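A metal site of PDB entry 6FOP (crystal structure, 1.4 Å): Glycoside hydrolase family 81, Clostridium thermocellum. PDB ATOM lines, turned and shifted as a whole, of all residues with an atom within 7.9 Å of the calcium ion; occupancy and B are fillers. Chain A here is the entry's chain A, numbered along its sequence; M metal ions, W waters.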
ATOM      1  N   PRO A  36      -5.217  -1.293 -11.053  1.00  0.00           N
ATOM      2  CA  PRO A  36      -5.258  -2.697 -10.665  1.00  0.00           C
ATOM      3  C   PRO A  36      -5.374  -2.894  -9.153  1.00  0.00           C
ATOM      4  O   PRO A  36      -4.753  -2.150  -8.374  1.00  0.00           O
ATOM      5  CB  PRO A  36      -3.913  -3.240 -11.181  1.00  0.00           C
ATOM      6  CG  PRO A  36      -3.597  -2.329 -12.318  1.00  0.00           C
ATOM      7  CD  PRO A  36      -4.034  -0.982 -11.867  1.00  0.00           C
ATOM      8  N   THR A  37      -6.175  -3.875  -8.753  1.00  0.00           N
ATOM      9  CA  THR A  37      -6.350  -4.265  -7.346  1.00  0.00           C
ATOM     10  C   THR A  37      -6.331  -5.785  -7.245  1.00  0.00           C
ATOM     11  O   THR A  37      -6.182  -6.503  -8.251  1.00  0.00           O
ATOM     12  CB  THR A  37      -7.698  -3.743  -6.806  1.00  0.00           C
ATOM     13  OG1 THR A  37      -8.785  -4.402  -7.461  1.00  0.00           O
ATOM     14  CG2 THR A  37      -7.846  -2.252  -7.021  1.00  0.00           C
ATOM     15  N   ASN A  38      -6.484  -6.305  -6.030  1.00  0.00           N
ATOM     16  CA  ASN A  38      -6.659  -7.734  -5.836  1.00  0.00           C
ATOM     17  C   ASN A  38      -5.486  -8.536  -6.354  1.00  0.00           C
ATOM     18  O   ASN A  38      -5.643  -9.556  -7.006  1.00  0.00           O
ATOM     19  CB  ASN A  38      -7.979  -8.280  -6.437  1.00  0.00           C
ATOM     20  CG  ASN A  38      -9.183  -7.640  -5.812  1.00  0.00           C
ATOM     21  OD1 ASN A  38      -9.670  -6.601  -6.268  1.00  0.00           O
ATOM     22  ND2 ASN A  38      -9.716  -8.282  -4.766  1.00  0.00           N
ATOM     23  N   SER A  39      -4.272  -8.045  -6.049  1.00  0.00           N
ATOM     24  CA  SER A  39      -3.093  -8.738  -6.520  1.00  0.00           C
ATOM     25  C   SER A  39      -1.971  -8.710  -5.463  1.00  0.00           C
ATOM     26  O   SER A  39      -2.133  -8.238  -4.338  1.00  0.00           O
ATOM     27  CB  SER A  39      -2.681  -8.104  -7.840  1.00  0.00           C
ATOM     28  OG  SER A  39      -1.659  -8.865  -8.505  1.00  0.00           O
ATOM     29  N   TRP A  40      -0.846  -9.275  -5.836  1.00  0.00           N
ATOM     30  CA  TRP A  40       0.288  -9.390  -4.928  1.00  0.00           C
ATOM     31  C   TRP A  40       1.016  -8.058  -4.708  1.00  0.00           C
ATOM     32  O   TRP A  40       1.642  -7.846  -3.688  1.00  0.00           O
ATOM     33  CB  TRP A  40       1.265 -10.448  -5.452  1.00  0.00           C
ATOM     34  CG  TRP A  40       1.749 -10.202  -6.853  1.00  0.00           C
ATOM     35  CD1 TRP A  40       1.138 -10.587  -8.017  1.00  0.00           C
ATOM     36  CD2 TRP A  40       2.935  -9.488  -7.249  1.00  0.00           C
ATOM     37  NE1 TRP A  40       1.824 -10.148  -9.100  1.00  0.00           N
ATOM     38  CE2 TRP A  40       2.968  -9.505  -8.665  1.00  0.00           C
ATOM     39  CE3 TRP A  40       4.003  -8.893  -6.547  1.00  0.00           C
ATOM     40  CZ2 TRP A  40       3.987  -8.897  -9.389  1.00  0.00           C
ATOM     41  CZ3 TRP A  40       5.009  -8.301  -7.279  1.00  0.00           C
ATOM     42  CH2 TRP A  40       5.016  -8.313  -8.686  1.00  0.00           C
ATOM     43  N   GLU A  41       0.919  -7.135  -5.659  1.00  0.00           N
ATOM     44  CA  GLU A  41       1.575  -5.831  -5.565  1.00  0.00           C
ATOM     45  C   GLU A  41       0.668  -4.757  -4.936  1.00  0.00           C
ATOM     46  O   GLU A  41       1.079  -3.621  -4.730  1.00  0.00           O
ATOM     47  CB  GLU A  41       2.067  -5.366  -6.931  1.00  0.00           C
ATOM     48  CG  GLU A  41       0.983  -4.792  -7.860  1.00  0.00           C
ATOM     49  CD  GLU A  41       0.009  -5.774  -8.452  1.00  0.00           C
ATOM     50  OE1 GLU A  41       0.301  -6.980  -8.482  1.00  0.00           O
ATOM     51  OE2 GLU A  41      -1.032  -5.287  -8.995  1.00  0.00           O
ATOM     52  N   SER A  42      -0.591  -5.104  -4.645  1.00  0.00           N
ATOM     53  CA  SER A  42      -1.617  -4.106  -4.382  1.00  0.00           C
ATOM     54  C   SER A  42      -1.376  -3.198  -3.213  1.00  0.00           C
ATOM     55  O   SER A  42      -1.842  -2.061  -3.227  1.00  0.00           O
ATOM     56  CB  SER A  42      -2.979  -4.785  -4.267  1.00  0.00           C
ATOM     57  OG  SER A  42      -3.297  -5.449  -5.464  1.00  0.00           O
ATOM     58  N   ILE A 107       2.001  -1.155 -13.692  1.00  0.00           N
ATOM     59  CA  ILE A 107       1.648  -2.512 -13.264  1.00  0.00           C
ATOM     60  C   ILE A 107       1.362  -3.292 -14.521  1.00  0.00           C
ATOM     61  O   ILE A 107       0.471  -2.930 -15.305  1.00  0.00           O
ATOM     62  CB  ILE A 107       0.471  -2.540 -12.285  1.00  0.00           C
ATOM     63  CG1 ILE A 107       0.810  -1.761 -11.004  1.00  0.00           C
ATOM     64  CG2 ILE A 107       0.133  -3.990 -11.960  1.00  0.00           C
ATOM     65  CD1 ILE A 107      -0.382  -1.527 -10.079  1.00  0.00           C
ATOM     66  N   SER A 108       2.147  -4.330 -14.757  1.00  0.00           N
ATOM     67  CA  SER A 108       1.931  -5.233 -15.879  1.00  0.00           C
ATOM     68  C   SER A 108       1.422  -6.588 -15.378  1.00  0.00           C
ATOM     69  O   SER A 108       1.012  -6.725 -14.215  1.00  0.00           O
ATOM     70  CB  SER A 108       3.177  -5.320 -16.753  1.00  0.00           C
ATOM     71  OG  SER A 108       4.280  -5.777 -16.007  1.00  0.00           O
ATOM     72  N   ASP A 109       1.451  -7.614 -16.234  1.00  0.00           N
ATOM     73  CA  ASP A 109       0.719  -8.833 -15.874  1.00  0.00           C
ATOM     74  C   ASP A 109       1.388  -9.631 -14.770  1.00  0.00           C
ATOM     75  O   ASP A 109       0.727 -10.400 -14.087  1.00  0.00           O
ATOM     76  CB  ASP A 109       0.488  -9.697 -17.127  1.00  0.00           C
ATOM     77  CG  ASP A 109      -0.509  -9.055 -18.127  1.00  0.00           C
ATOM     78  OD1 ASP A 109      -1.089  -8.006 -17.856  1.00  0.00           O
ATOM     79  OD2 ASP A 109      -0.680  -9.643 -19.183  1.00  0.00           O
ATOM     80  N   ILE A 454     -14.532  -7.892 -12.893  1.00  0.00           N
ATOM     81  CA  ILE A 454     -13.740  -8.949 -12.272  1.00  0.00           C
ATOM     82  C   ILE A 454     -12.679  -9.553 -13.172  1.00  0.00           C
ATOM     83  O   ILE A 454     -11.702 -10.105 -12.669  1.00  0.00           O
ATOM     84  CB  ILE A 454     -14.615 -10.069 -11.703  1.00  0.00           C
ATOM     85  CG1 ILE A 454     -15.373 -10.870 -12.797  1.00  0.00           C
ATOM     86  CG2 ILE A 454     -15.568  -9.465 -10.669  1.00  0.00           C
ATOM     87  CD1 ILE A 454     -16.157 -12.052 -12.241  1.00  0.00           C
ATOM     88  N   PRO A 465      -9.542  -2.381 -14.671  1.00  0.00           N
ATOM     89  CA  PRO A 465      -8.187  -2.859 -14.889  1.00  0.00           C
ATOM     90  C   PRO A 465      -8.203  -4.243 -15.547  1.00  0.00           C
ATOM     91  O   PRO A 465      -9.242  -4.926 -15.555  1.00  0.00           O
ATOM     92  CB  PRO A 465      -7.611  -2.907 -13.481  1.00  0.00           C
ATOM     93  CG  PRO A 465      -8.791  -3.254 -12.619  1.00  0.00           C
ATOM     94  CD  PRO A 465      -9.981  -2.582 -13.274  1.00  0.00           C
ATOM     95  N   PHE A 466      -7.076  -4.660 -16.102  1.00  0.00           N
ATOM     96  CA  PHE A 466      -6.959  -5.944 -16.783  1.00  0.00           C
ATOM     97  C   PHE A 466      -7.010  -7.078 -15.770  1.00  0.00           C
ATOM     98  O   PHE A 466      -6.223  -7.098 -14.818  1.00  0.00           O
ATOM     99  CB  PHE A 466      -5.655  -5.991 -17.557  1.00  0.00           C
ATOM    100  CG  PHE A 466      -5.476  -7.227 -18.392  1.00  0.00           C
ATOM    101  CD1 PHE A 466      -6.201  -7.411 -19.555  1.00  0.00           C
ATOM    102  CD2 PHE A 466      -4.511  -8.155 -18.066  1.00  0.00           C
ATOM    103  CE1 PHE A 466      -6.007  -8.539 -20.320  1.00  0.00           C
ATOM    104  CE2 PHE A 466      -4.306  -9.279 -18.843  1.00  0.00           C
ATOM    105  CZ  PHE A 466      -5.052  -9.456 -19.961  1.00  0.00           C
ATOM    106  N   LEU A 467      -7.958  -7.994 -15.930  1.00  0.00           N
ATOM    107  CA  LEU A 467      -8.060  -9.206 -15.105  1.00  0.00           C
ATOM    108  C   LEU A 467      -7.917  -8.954 -13.619  1.00  0.00           C
ATOM    109  O   LEU A 467      -6.963  -9.430 -12.963  1.00  0.00           O
ATOM    110  CB  LEU A 467      -7.052 -10.272 -15.580  1.00  0.00           C
ATOM    111  CG  LEU A 467      -7.142 -10.798 -17.004  1.00  0.00           C
ATOM    112  CD1 LEU A 467      -6.092 -11.872 -17.225  1.00  0.00           C
ATOM    113  CD2 LEU A 467      -8.552 -11.318 -17.334  1.00  0.00           C
ATOM    114  N   ARG A 468      -8.876  -8.224 -13.062  1.00  0.00           N
ATOM    115  CA  ARG A 468      -8.777  -7.843 -11.664  1.00  0.00           C
ATOM    116  C   ARG A 468      -8.434  -8.982 -10.717  1.00  0.00           C
ATOM    117  O   ARG A 468      -7.325  -9.052 -10.165  1.00  0.00           O
ATOM    118  CB  ARG A 468     -10.028  -7.106 -11.159  1.00  0.00           C
ATOM    119  CG  ARG A 468      -9.877  -6.539  -9.758  1.00  0.00           C
ATOM    120  CD  ARG A 468     -11.177  -6.088  -9.129  1.00  0.00           C
ATOM    121  NE  ARG A 468     -11.878  -5.154  -9.987  1.00  0.00           N
ATOM    122  CZ  ARG A 468     -11.620  -3.847 -10.072  1.00  0.00           C
ATOM    123  NH1 ARG A 468     -10.649  -3.264  -9.358  1.00  0.00           N
ATOM    124  NH2 ARG A 468     -12.301  -3.104 -10.941  1.00  0.00           N
ATOM    125  N   ASN A 469      -9.378  -9.908 -10.493  1.00  0.00           N
ATOM    126  CA  ASN A 469      -9.127 -10.894  -9.435  1.00  0.00           C
ATOM    127  C   ASN A 469      -8.114 -11.979  -9.776  1.00  0.00           C
ATOM    128  O   ASN A 469      -7.431 -12.490  -8.875  1.00  0.00           O
ATOM    129  CB  ASN A 469     -10.429 -11.493  -8.935  1.00  0.00           C
ATOM    130  CG  ASN A 469     -11.262 -10.449  -8.232  1.00  0.00           C
ATOM    131  OD1 ASN A 469     -12.087  -9.782  -8.886  1.00  0.00           O
ATOM    132  ND2 ASN A 469     -11.063 -10.257  -6.946  1.00  0.00           N
ATOM    133  N   PHE A 470      -7.964 -12.297 -11.065  1.00  0.00           N
ATOM    134  CA  PHE A 470      -7.088 -13.388 -11.467  1.00  0.00           C
ATOM    135  C   PHE A 470      -5.641 -12.916 -11.508  1.00  0.00           C
ATOM    136  O   PHE A 470      -5.382 -11.835 -12.052  1.00  0.00           O
ATOM    137  CB  PHE A 470      -7.483 -13.929 -12.821  1.00  0.00           C
ATOM    138  CG  PHE A 470      -6.813 -15.223 -13.178  1.00  0.00           C
ATOM    139  CD1 PHE A 470      -7.145 -16.397 -12.485  1.00  0.00           C
ATOM    140  CD2 PHE A 470      -5.900 -15.309 -14.199  1.00  0.00           C
ATOM    141  CE1 PHE A 470      -6.549 -17.600 -12.801  1.00  0.00           C
ATOM    142  CE2 PHE A 470      -5.315 -16.510 -14.524  1.00  0.00           C
ATOM    143  CZ  PHE A 470      -5.647 -17.666 -13.818  1.00  0.00           C
ATOM    144  N   ASP A 471      -4.712 -13.729 -10.999  1.00  0.00           N
ATOM    145  CA  ASP A 471      -3.247 -13.480 -11.083  1.00  0.00           C
ATOM    146  C   ASP A 471      -2.732 -14.429 -12.179  1.00  0.00           C
ATOM    147  O   ASP A 471      -2.693 -15.658 -11.985  1.00  0.00           O
ATOM    148  CB  ASP A 471      -2.626 -13.799  -9.745  1.00  0.00           C
ATOM    149  CG  ASP A 471      -1.113 -13.588  -9.694  1.00  0.00           C
ATOM    150  OD1 ASP A 471      -0.456 -13.810 -10.737  1.00  0.00           O
ATOM    151  OD2 ASP A 471      -0.613 -13.307  -8.575  1.00  0.00           O
ATOM    152  N   PRO A 472      -2.353 -13.881 -13.329  1.00  0.00           N
ATOM    153  CA  PRO A 472      -1.959 -14.765 -14.439  1.00  0.00           C
ATOM    154  C   PRO A 472      -0.765 -15.664 -14.170  1.00  0.00           C
ATOM    155  O   PRO A 472      -0.613 -16.716 -14.813  1.00  0.00           O
ATOM    156  CB  PRO A 472      -1.669 -13.798 -15.594  1.00  0.00           C
ATOM    157  CG  PRO A 472      -2.319 -12.528 -15.208  1.00  0.00           C
ATOM    158  CD  PRO A 472      -2.361 -12.464 -13.734  1.00  0.00           C
ATOM    159  N   HIS A 476      -4.110 -18.312 -10.170  1.00  0.00           N
ATOM    160  CA  HIS A 476      -5.311 -18.357  -9.382  1.00  0.00           C
ATOM    161  C   HIS A 476      -5.726 -16.941  -9.036  1.00  0.00           C
ATOM    162  O   HIS A 476      -4.955 -15.978  -9.295  1.00  0.00           O
ATOM    163  CB  HIS A 476      -5.124 -19.184  -8.093  1.00  0.00           C
ATOM    164  CG  HIS A 476      -4.158 -18.582  -7.143  1.00  0.00           C
ATOM    165  ND1 HIS A 476      -4.497 -17.569  -6.276  1.00  0.00           N
ATOM    166  CD2 HIS A 476      -2.813 -18.771  -7.005  1.00  0.00           C
ATOM    167  CE1 HIS A 476      -3.411 -17.147  -5.646  1.00  0.00           C
ATOM    168  NE2 HIS A 476      -2.386 -17.887  -6.052  1.00  0.00           N
ATOM    169  N   SER A 477      -6.851 -16.797  -8.371  1.00  0.00           N
ATOM    170  CA  SER A 477      -7.377 -15.529  -7.977  1.00  0.00           C
ATOM    171  C   SER A 477      -7.010 -15.097  -6.580  1.00  0.00           C
ATOM    172  O   SER A 477      -6.547 -15.914  -5.749  1.00  0.00           O
ATOM    173  CB  SER A 477      -8.876 -15.523  -8.216  1.00  0.00           C
ATOM    174  OG  SER A 477      -9.179 -15.779  -9.571  1.00  0.00           O
ATOM    175  N   TRP A 478      -7.248 -13.810  -6.311  1.00  0.00           N
ATOM    176  CA  TRP A 478      -6.973 -13.214  -5.028  1.00  0.00           C
ATOM    177  C   TRP A 478      -8.214 -12.478  -4.514  1.00  0.00           C
ATOM    178  O   TRP A 478      -8.893 -11.743  -5.266  1.00  0.00           O
ATOM    179  CB  TRP A 478      -5.849 -12.208  -5.128  1.00  0.00           C
ATOM    180  CG  TRP A 478      -4.467 -12.752  -5.385  1.00  0.00           C
ATOM    181  CD1 TRP A 478      -3.680 -12.446  -6.457  1.00  0.00           C
ATOM    182  CD2 TRP A 478      -3.673 -13.598  -4.549  1.00  0.00           C
ATOM    183  NE1 TRP A 478      -2.455 -13.054  -6.366  1.00  0.00           N
ATOM    184  CE2 TRP A 478      -2.425 -13.766  -5.197  1.00  0.00           C
ATOM    185  CE3 TRP A 478      -3.892 -14.274  -3.349  1.00  0.00           C
ATOM    186  CZ2 TRP A 478      -1.391 -14.486  -4.636  1.00  0.00           C
ATOM    187  CZ3 TRP A 478      -2.858 -14.993  -2.789  1.00  0.00           C
ATOM    188  CH2 TRP A 478      -1.631 -15.113  -3.460  1.00  0.00           C
HETATM  189 CA    CA M   1      -5.241  -9.610 -11.408  1.00  0.00          CA
HETATM  190  O   HOH W   1      -2.855  -9.906 -11.022  1.00  0.00           O
HETATM  191  O   HOH W   2      -4.923  -7.412 -10.527  1.00  0.00           O
HETATM  192  O   HOH W   3      -4.335  -8.655 -13.405  1.00  0.00           O
HETATM  193  O   HOH W   4      -5.071 -10.777  -9.289  1.00  0.00           O
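Within 4 Å of the calcium ion: Leu 467, Arg 468 and Phe 470.
The backbone carbonyl oxygen (O) of Phe 470 is bound to the calcium ion (2.3 Å).
O of Leu 467 is bound to the calcium ion.
Water W2 is bound to the calcium ion, at 2.4 Å.
Water W3 is bound to the calcium ion.
The calcium ion is bound by water W4 (2.4 Å).
The calcium ion is bound by water W1, 2.4 Å away.
The backbone carbonyl oxygen (O) of Arg 468 binds the calcium ion.
Water W4 lies within hydrogen-bond range of O of Asn 38 (2.7 Å), O of Asn 469 (2.9 Å) and N of Asp 471 (3.4 Å).
The side-chain hydroxyl of Thr 37 sits at hydrogen-bond distance from the guanidinium group of Arg 468, at 2.9 Å.
N of Arg 468 lies within hydrogen-bond range of O of Ile 454 (3.4 Å).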
